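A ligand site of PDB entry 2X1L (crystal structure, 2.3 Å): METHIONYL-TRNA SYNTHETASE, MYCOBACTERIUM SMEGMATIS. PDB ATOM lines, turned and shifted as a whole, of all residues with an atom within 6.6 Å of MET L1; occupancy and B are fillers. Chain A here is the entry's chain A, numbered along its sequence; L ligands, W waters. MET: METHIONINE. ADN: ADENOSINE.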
ATOM      1  N   THR A  18       8.648 -16.451  10.590  1.00  0.00           N
ATOM      2  CA  THR A  18       7.200 -16.511  10.709  1.00  0.00           C
ATOM      3  C   THR A  18       6.647 -15.100  10.527  1.00  0.00           C
ATOM      4  O   THR A  18       7.374 -14.118  10.651  1.00  0.00           O
ATOM      5  CB  THR A  18       6.725 -17.057  12.077  1.00  0.00           C
ATOM      6  OG1 THR A  18       6.980 -16.094  13.100  1.00  0.00           O
ATOM      7  CG2 THR A  18       7.432 -18.349  12.423  1.00  0.00           C
ATOM      8  N   ALA A  19       5.353 -15.011  10.228  1.00  0.00           N
ATOM      9  CA  ALA A  19       4.647 -13.736  10.282  1.00  0.00           C
ATOM     10  C   ALA A  19       4.646 -13.249  11.716  1.00  0.00           C
ATOM     11  O   ALA A  19       4.574 -14.045  12.656  1.00  0.00           O
ATOM     12  CB  ALA A  19       3.227 -13.905   9.775  1.00  0.00           C
ATOM     13  N   ILE A  20       4.755 -11.939  11.896  1.00  0.00           N
ATOM     14  CA  ILE A  20       4.745 -11.331  13.222  1.00  0.00           C
ATOM     15  C   ILE A  20       3.341 -10.820  13.571  1.00  0.00           C
ATOM     16  O   ILE A  20       2.820  -9.910  12.917  1.00  0.00           O
ATOM     17  CB  ILE A  20       5.825 -10.229  13.374  1.00  0.00           C
ATOM     18  CG1 ILE A  20       5.766  -9.235  12.214  1.00  0.00           C
ATOM     19  CG2 ILE A  20       7.218 -10.873  13.451  1.00  0.00           C
ATOM     20  CD1 ILE A  20       6.541  -7.953  12.437  1.00  0.00           C
ATOM     21  N   ALA A  21       2.721 -11.424  14.586  1.00  0.00           N
ATOM     22  CA  ALA A  21       1.322 -11.171  14.913  1.00  0.00           C
ATOM     23  C   ALA A  21       1.078  -9.828  15.599  1.00  0.00           C
ATOM     24  O   ALA A  21       1.949  -9.322  16.320  1.00  0.00           O
ATOM     25  CB  ALA A  21       0.773 -12.290  15.781  1.00  0.00           C
ATOM     26  N   TYR A  22      -0.098  -9.255  15.362  1.00  0.00           N
ATOM     27  CA  TYR A  22      -0.576  -8.136  16.175  1.00  0.00           C
ATOM     28  C   TYR A  22      -0.932  -8.702  17.556  1.00  0.00           C
ATOM     29  O   TYR A  22      -1.760  -9.613  17.650  1.00  0.00           O
ATOM     30  CB  TYR A  22      -1.830  -7.488  15.567  1.00  0.00           C
ATOM     31  CG  TYR A  22      -1.662  -6.912  14.183  1.00  0.00           C
ATOM     32  CD1 TYR A  22      -2.413  -7.412  13.111  1.00  0.00           C
ATOM     33  CD2 TYR A  22      -0.771  -5.859  13.927  1.00  0.00           C
ATOM     34  CE1 TYR A  22      -2.283  -6.884  11.829  1.00  0.00           C
ATOM     35  CE2 TYR A  22      -0.632  -5.335  12.642  1.00  0.00           C
ATOM     36  CZ  TYR A  22      -1.391  -5.852  11.608  1.00  0.00           C
ATOM     37  OH  TYR A  22      -1.254  -5.342  10.338  1.00  0.00           O
ATOM     38  N   HIS A  31      -2.044 -19.183  15.835  1.00  0.00           N
ATOM     39  CA  HIS A  31      -0.671 -18.717  16.063  1.00  0.00           C
ATOM     40  C   HIS A  31       0.245 -19.899  16.377  1.00  0.00           C
ATOM     41  O   HIS A  31       1.304 -20.054  15.761  1.00  0.00           O
ATOM     42  CB  HIS A  31      -0.619 -17.699  17.205  1.00  0.00           C
ATOM     43  CG  HIS A  31      -1.389 -16.446  16.938  1.00  0.00           C
ATOM     44  ND1 HIS A  31      -2.507 -16.083  17.661  1.00  0.00           N
ATOM     45  CD2 HIS A  31      -1.206 -15.466  16.024  1.00  0.00           C
ATOM     46  CE1 HIS A  31      -2.966 -14.927  17.208  1.00  0.00           C
ATOM     47  NE2 HIS A  31      -2.197 -14.532  16.211  1.00  0.00           N
ATOM     48  N   THR A  58       6.465 -10.081  17.119  1.00  0.00           N
ATOM     49  CA  THR A  58       5.202  -9.333  17.146  1.00  0.00           C
ATOM     50  C   THR A  58       5.248  -8.025  16.356  1.00  0.00           C
ATOM     51  O   THR A  58       6.286  -7.373  16.254  1.00  0.00           O
ATOM     52  CB  THR A  58       4.728  -9.028  18.587  1.00  0.00           C
ATOM     53  OG1 THR A  58       5.765  -8.354  19.311  1.00  0.00           O
ATOM     54  CG2 THR A  58       4.342 -10.309  19.325  1.00  0.00           C
ATOM     55  N   ASP A  59       4.093  -7.654  15.818  1.00  0.00           N
ATOM     56  CA  ASP A  59       3.888  -6.439  15.043  1.00  0.00           C
ATOM     57  C   ASP A  59       3.058  -5.476  15.892  1.00  0.00           C
ATOM     58  O   ASP A  59       1.835  -5.620  15.979  1.00  0.00           O
ATOM     59  CB  ASP A  59       3.145  -6.809  13.750  1.00  0.00           C
ATOM     60  CG  ASP A  59       2.994  -5.658  12.782  1.00  0.00           C
ATOM     61  OD1 ASP A  59       3.546  -4.557  13.022  1.00  0.00           O
ATOM     62  OD2 ASP A  59       2.322  -5.851  11.750  1.00  0.00           O
ATOM     63  N   LYS A  64      -5.238  -0.592  14.715  1.00  0.00           N
ATOM     64  CA  LYS A  64      -5.861  -1.720  15.411  1.00  0.00           C
ATOM     65  C   LYS A  64      -5.333  -1.844  16.842  1.00  0.00           C
ATOM     66  O   LYS A  64      -6.112  -2.015  17.772  1.00  0.00           O
ATOM     67  CB  LYS A  64      -5.656  -3.020  14.635  1.00  0.00           C
ATOM     68  CG  LYS A  64      -6.506  -4.194  15.115  1.00  0.00           C
ATOM     69  CD  LYS A  64      -6.185  -5.459  14.334  1.00  0.00           C
ATOM     70  CE  LYS A  64      -7.186  -6.555  14.630  1.00  0.00           C
ATOM     71  NZ  LYS A  64      -6.893  -7.799  13.878  1.00  0.00           N
ATOM     72  N   ASP A 139      -8.209  -5.322   9.352  1.00  0.00           N
ATOM     73  CA  ASP A 139      -7.295  -5.942   8.383  1.00  0.00           C
ATOM     74  C   ASP A 139      -6.012  -5.131   8.176  1.00  0.00           C
ATOM     75  O   ASP A 139      -5.050  -5.627   7.595  1.00  0.00           O
ATOM     76  CB  ASP A 139      -7.999  -6.146   7.045  1.00  0.00           C
ATOM     77  CG  ASP A 139      -9.218  -7.052   7.142  1.00  0.00           C
ATOM     78  OD1 ASP A 139      -9.065  -8.209   7.591  1.00  0.00           O
ATOM     79  OD2 ASP A 139     -10.321  -6.610   6.763  1.00  0.00           O
ATOM     80  N   VAL A 238       1.677   0.572   8.744  1.00  0.00           N
ATOM     81  CA  VAL A 238       2.080  -0.538   9.621  1.00  0.00           C
ATOM     82  C   VAL A 238       2.748  -1.703   8.875  1.00  0.00           C
ATOM     83  O   VAL A 238       3.660  -2.333   9.394  1.00  0.00           O
ATOM     84  CB  VAL A 238       0.902  -1.016  10.534  1.00  0.00           C
ATOM     85  CG1 VAL A 238      -0.256  -1.599   9.713  1.00  0.00           C
ATOM     86  CG2 VAL A 238       1.382  -2.010  11.588  1.00  0.00           C
ATOM     87  N   TRP A 239       2.288  -1.959   7.648  1.00  0.00           N
ATOM     88  CA  TRP A 239       2.807  -3.063   6.840  1.00  0.00           C
ATOM     89  C   TRP A 239       4.227  -2.883   6.304  1.00  0.00           C
ATOM     90  O   TRP A 239       5.007  -3.833   6.278  1.00  0.00           O
ATOM     91  CB  TRP A 239       1.822  -3.428   5.725  1.00  0.00           C
ATOM     92  CG  TRP A 239       0.778  -4.380   6.207  1.00  0.00           C
ATOM     93  CD1 TRP A 239      -0.503  -4.074   6.588  1.00  0.00           C
ATOM     94  CD2 TRP A 239       0.914  -5.791   6.384  1.00  0.00           C
ATOM     95  NE1 TRP A 239      -1.168  -5.208   6.980  1.00  0.00           N
ATOM     96  CE2 TRP A 239      -0.319  -6.277   6.865  1.00  0.00           C
ATOM     97  CE3 TRP A 239       1.966  -6.698   6.175  1.00  0.00           C
ATOM     98  CZ2 TRP A 239      -0.537  -7.632   7.141  1.00  0.00           C
ATOM     99  CZ3 TRP A 239       1.749  -8.045   6.444  1.00  0.00           C
ATOM    100  CH2 TRP A 239       0.509  -8.498   6.928  1.00  0.00           C
ATOM    101  N   ALA A 242       6.162  -3.435   9.323  1.00  0.00           N
ATOM    102  CA  ALA A 242       6.095  -4.850   9.674  1.00  0.00           C
ATOM    103  C   ALA A 242       6.950  -5.757   8.785  1.00  0.00           C
ATOM    104  O   ALA A 242       7.660  -6.632   9.291  1.00  0.00           O
ATOM    105  CB  ALA A 242       4.651  -5.335   9.668  1.00  0.00           C
ATOM    106  N   LEU A 243       6.874  -5.550   7.472  1.00  0.00           N
ATOM    107  CA  LEU A 243       7.604  -6.353   6.495  1.00  0.00           C
ATOM    108  C   LEU A 243       9.125  -6.247   6.652  1.00  0.00           C
ATOM    109  O   LEU A 243       9.841  -7.207   6.372  1.00  0.00           O
ATOM    110  CB  LEU A 243       7.200  -5.951   5.070  1.00  0.00           C
ATOM    111  CG  LEU A 243       6.199  -6.786   4.241  1.00  0.00           C
ATOM    112  CD1 LEU A 243       5.329  -7.732   5.059  1.00  0.00           C
ATOM    113  CD2 LEU A 243       5.348  -5.877   3.370  1.00  0.00           C
ATOM    114  N   THR A 244       9.589  -5.096   7.107  1.00  0.00           N
ATOM    115  CA  THR A 244      11.010  -4.816   7.276  1.00  0.00           C
ATOM    116  C   THR A 244      11.656  -5.637   8.407  1.00  0.00           C
ATOM    117  O   THR A 244      12.874  -5.753   8.476  1.00  0.00           O
ATOM    118  CB  THR A 244      11.268  -3.297   7.495  1.00  0.00           C
ATOM    119  OG1 THR A 244      10.647  -2.560   6.427  1.00  0.00           O
ATOM    120  CG2 THR A 244      12.754  -2.969   7.498  1.00  0.00           C
ATOM    121  N   ASN A 245      10.831  -6.231   9.277  1.00  0.00           N
ATOM    122  CA  ASN A 245      11.343  -7.059  10.382  1.00  0.00           C
ATOM    123  C   ASN A 245      12.216  -8.211   9.914  1.00  0.00           C
ATOM    124  O   ASN A 245      13.166  -8.595  10.590  1.00  0.00           O
ATOM    125  CB  ASN A 245      10.199  -7.560  11.293  1.00  0.00           C
ATOM    126  CG  ASN A 245       9.684  -8.925  10.876  1.00  0.00           C
ATOM    127  OD1 ASN A 245      10.058  -9.946  11.459  1.00  0.00           O
ATOM    128  ND2 ASN A 245       8.811  -8.954   9.874  1.00  0.00           N
ATOM    129  N   TYR A 246      11.902  -8.750   8.731  1.00  0.00           N
ATOM    130  CA  TYR A 246      12.662  -9.846   8.133  1.00  0.00           C
ATOM    131  C   TYR A 246      14.100  -9.423   7.802  1.00  0.00           C
ATOM    132  O   TYR A 246      15.009 -10.259   7.778  1.00  0.00           O
ATOM    133  CB  TYR A 246      11.960 -10.371   6.865  1.00  0.00           C
ATOM    134  CG  TYR A 246      10.532 -10.850   7.074  1.00  0.00           C
ATOM    135  CD1 TYR A 246      10.209 -11.701   8.133  1.00  0.00           C
ATOM    136  CD2 TYR A 246       9.515 -10.465   6.196  1.00  0.00           C
ATOM    137  CE1 TYR A 246       8.901 -12.149   8.320  1.00  0.00           C
ATOM    138  CE2 TYR A 246       8.203 -10.919   6.377  1.00  0.00           C
ATOM    139  CZ  TYR A 246       7.899 -11.755   7.439  1.00  0.00           C
ATOM    140  OH  TYR A 246       6.614 -12.204   7.628  1.00  0.00           O
ATOM    141  N   ILE A 271       3.817 -17.938   6.373  1.00  0.00           N
ATOM    142  CA  ILE A 271       2.664 -17.062   6.635  1.00  0.00           C
ATOM    143  C   ILE A 271       1.358 -17.818   6.419  1.00  0.00           C
ATOM    144  O   ILE A 271       1.341 -18.897   5.834  1.00  0.00           O
ATOM    145  CB  ILE A 271       2.665 -15.804   5.722  1.00  0.00           C
ATOM    146  CG1 ILE A 271       2.605 -16.198   4.242  1.00  0.00           C
ATOM    147  CG2 ILE A 271       3.864 -14.906   6.016  1.00  0.00           C
ATOM    148  CD1 ILE A 271       2.004 -15.144   3.353  1.00  0.00           C
ATOM    149  N   ASP A 274      -4.201 -15.382   4.618  1.00  0.00           N
ATOM    150  CA  ASP A 274      -4.899 -14.100   4.736  1.00  0.00           C
ATOM    151  C   ASP A 274      -3.984 -12.886   4.512  1.00  0.00           C
ATOM    152  O   ASP A 274      -4.469 -11.774   4.319  1.00  0.00           O
ATOM    153  CB  ASP A 274      -5.628 -13.985   6.085  1.00  0.00           C
ATOM    154  CG  ASP A 274      -4.672 -14.042   7.281  1.00  0.00           C
ATOM    155  OD1 ASP A 274      -3.637 -14.742   7.211  1.00  0.00           O
ATOM    156  OD2 ASP A 274      -4.966 -13.376   8.302  1.00  0.00           O
ATOM    157  N   ILE A 275      -2.677 -13.111   4.545  1.00  0.00           N
ATOM    158  CA  ILE A 275      -1.701 -12.028   4.386  1.00  0.00           C
ATOM    159  C   ILE A 275      -0.726 -12.269   3.231  1.00  0.00           C
ATOM    160  O   ILE A 275       0.391 -11.739   3.205  1.00  0.00           O
ATOM    161  CB  ILE A 275      -0.935 -11.728   5.713  1.00  0.00           C
ATOM    162  CG1 ILE A 275      -0.247 -12.994   6.233  1.00  0.00           C
ATOM    163  CG2 ILE A 275      -1.889 -11.141   6.756  1.00  0.00           C
ATOM    164  CD1 ILE A 275       0.746 -12.747   7.362  1.00  0.00           C
ATOM    165  N   HIS A 279       3.019 -10.195   1.254  1.00  0.00           N
ATOM    166  CA  HIS A 279       4.305 -10.873   1.159  1.00  0.00           C
ATOM    167  C   HIS A 279       4.736 -11.204  -0.272  1.00  0.00           C
ATOM    168  O   HIS A 279       5.927 -11.350  -0.542  1.00  0.00           O
ATOM    169  CB  HIS A 279       4.290 -12.144   2.002  1.00  0.00           C
ATOM    170  CG  HIS A 279       4.345 -11.887   3.476  1.00  0.00           C
ATOM    171  ND1 HIS A 279       3.218 -11.611   4.225  1.00  0.00           N
ATOM    172  CD2 HIS A 279       5.385 -11.852   4.341  1.00  0.00           C
ATOM    173  CE1 HIS A 279       3.567 -11.422   5.484  1.00  0.00           C
ATOM    174  NE2 HIS A 279       4.871 -11.565   5.580  1.00  0.00           N
HETATM  175  N   MET L   1       0.731  -8.435  11.919  1.00  0.00           N
HETATM  176  CA  MET L   1       0.244  -9.206  10.768  1.00  0.00           C
HETATM  177  C   MET L   1      -0.916 -10.113  11.164  1.00  0.00           C
HETATM  178  O   MET L   1      -1.671 -10.577  10.308  1.00  0.00           O
HETATM  179  CB  MET L   1       1.380 -10.039  10.169  1.00  0.00           C
HETATM  180  CG  MET L   1       2.578  -9.236   9.707  1.00  0.00           C
HETATM  181  SD  MET L   1       3.837 -10.270   8.936  1.00  0.00           S
HETATM  182  CE  MET L   1       5.060  -9.045   8.503  1.00  0.00           C
HETATM  183  OXT MET L   1      -1.137 -10.401  12.344  1.00  0.00           O
HETATM  184  O5' ADN L   2      -1.055 -13.504  12.957  1.00  0.00           O
HETATM  185  C5' ADN L   2       0.194 -14.103  12.598  1.00  0.00           C
HETATM  186  C4' ADN L   2      -0.036 -15.345  11.744  1.00  0.00           C
HETATM  187  O4' ADN L   2      -0.965 -16.247  12.360  1.00  0.00           O
HETATM  188  C3' ADN L   2      -0.588 -15.000  10.367  1.00  0.00           C
HETATM  189  O3' ADN L   2       0.284 -15.512   9.356  1.00  0.00           O
HETATM  190  C2' ADN L   2      -1.949 -15.677  10.316  1.00  0.00           C
HETATM  191  O2' ADN L   2      -2.219 -16.225   9.019  1.00  0.00           O
HETATM  192  C1' ADN L   2      -1.849 -16.763  11.365  1.00  0.00           C
HETATM  193  N9  ADN L   2      -3.189 -17.107  11.924  1.00  0.00           N
HETATM  194  C8  ADN L   2      -3.969 -16.302  12.673  1.00  0.00           C
HETATM  195  N7  ADN L   2      -5.134 -16.926  13.005  1.00  0.00           N
HETATM  196  C5  ADN L   2      -5.112 -18.150  12.468  1.00  0.00           C
HETATM  197  C6  ADN L   2      -6.017 -19.329  12.422  1.00  0.00           C
HETATM  198  N6  ADN L   2      -7.218 -19.305  13.060  1.00  0.00           N
HETATM  199  N1  ADN L   2      -5.606 -20.427  11.744  1.00  0.00           N
HETATM  200  C2  ADN L   2      -4.411 -20.464  11.106  1.00  0.00           C
HETATM  201  N3  ADN L   2      -3.540 -19.435  11.102  1.00  0.00           N
HETATM  202  C4  ADN L   2      -3.827 -18.268  11.753  1.00  0.00           C
HETATM  203  O   HOH W   1      -3.114 -11.937  14.146  1.00  0.00           O
HETATM  204  O   HOH W   2      -3.325 -12.602  10.332  1.00  0.00           O
HETATM  205  O   HOH W   3      -3.885  -9.273   9.420  1.00  0.00           O
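Merely in contact with MET L1: Trp 239, Ile 275, Ala 242, Ala 21, Leu 243, Ala 19 and Asn 245.
The nearest printed residue that does not touch MET L1 is Asp 274 (4.8 Å).
Water W2 lies within hydrogen-bond range of O of MET L1 (2.6 Å) and OD2 of Asp 274 (2.7 Å).
Water W1 lies within hydrogen-bond range of O5' of ADN L2 (2.8 Å), OXT of MET L1 (3.1 Å) and NE2 of His 31 (3.4 Å).
An oxygen (OXT) of MET L1 is in hydrogen-bond range of an oxygen (O5') of ADN L2 (3.2 Å).
SD of MET L1 sits close to N of Ile 20 (3.5 Å).
O of Ile 20 lies within hydrogen-bond range of N of MET L1, at 2.7 Å.
OD2 of Asp 59 lies within salt-bridge range of N of MET L1 (3.0 Å).
The backbone NH (N) of Tyr 22 lies close to an oxygen (OXT) of MET L1.
A sulfur (SD) of MET L1 sits close to the side-chain hydroxyl of Tyr 246, at 3.6 Å.
NE2 of His 279 lies close to SD of MET L1 (3.7 Å).
The side-chain carboxylate (OD1) of Asp 274 is in hydrogen-bond range of an oxygen (O2') of ADN L2.
N of Asp 59 lies within hydrogen-bond range of O of Ala 21 (2.8 Å).
NE1 of Trp 239 is in hydrogen-bond range of OH of Tyr 22, at 3.4 Å.
The backbone carbonyl oxygen of Ile 275 sits at hydrogen-bond distance from a ring nitrogen (ND1) of His 279.
A ring nitrogen (NE2) of His 279 lies within hydrogen-bond range of the side-chain hydroxyl of Tyr 246 (2.8 Å).
The side-chain amide nitrogen (ND2) of Asn 245 lies within hydrogen-bond range of the backbone carbonyl oxygen (O) of Ala 242.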
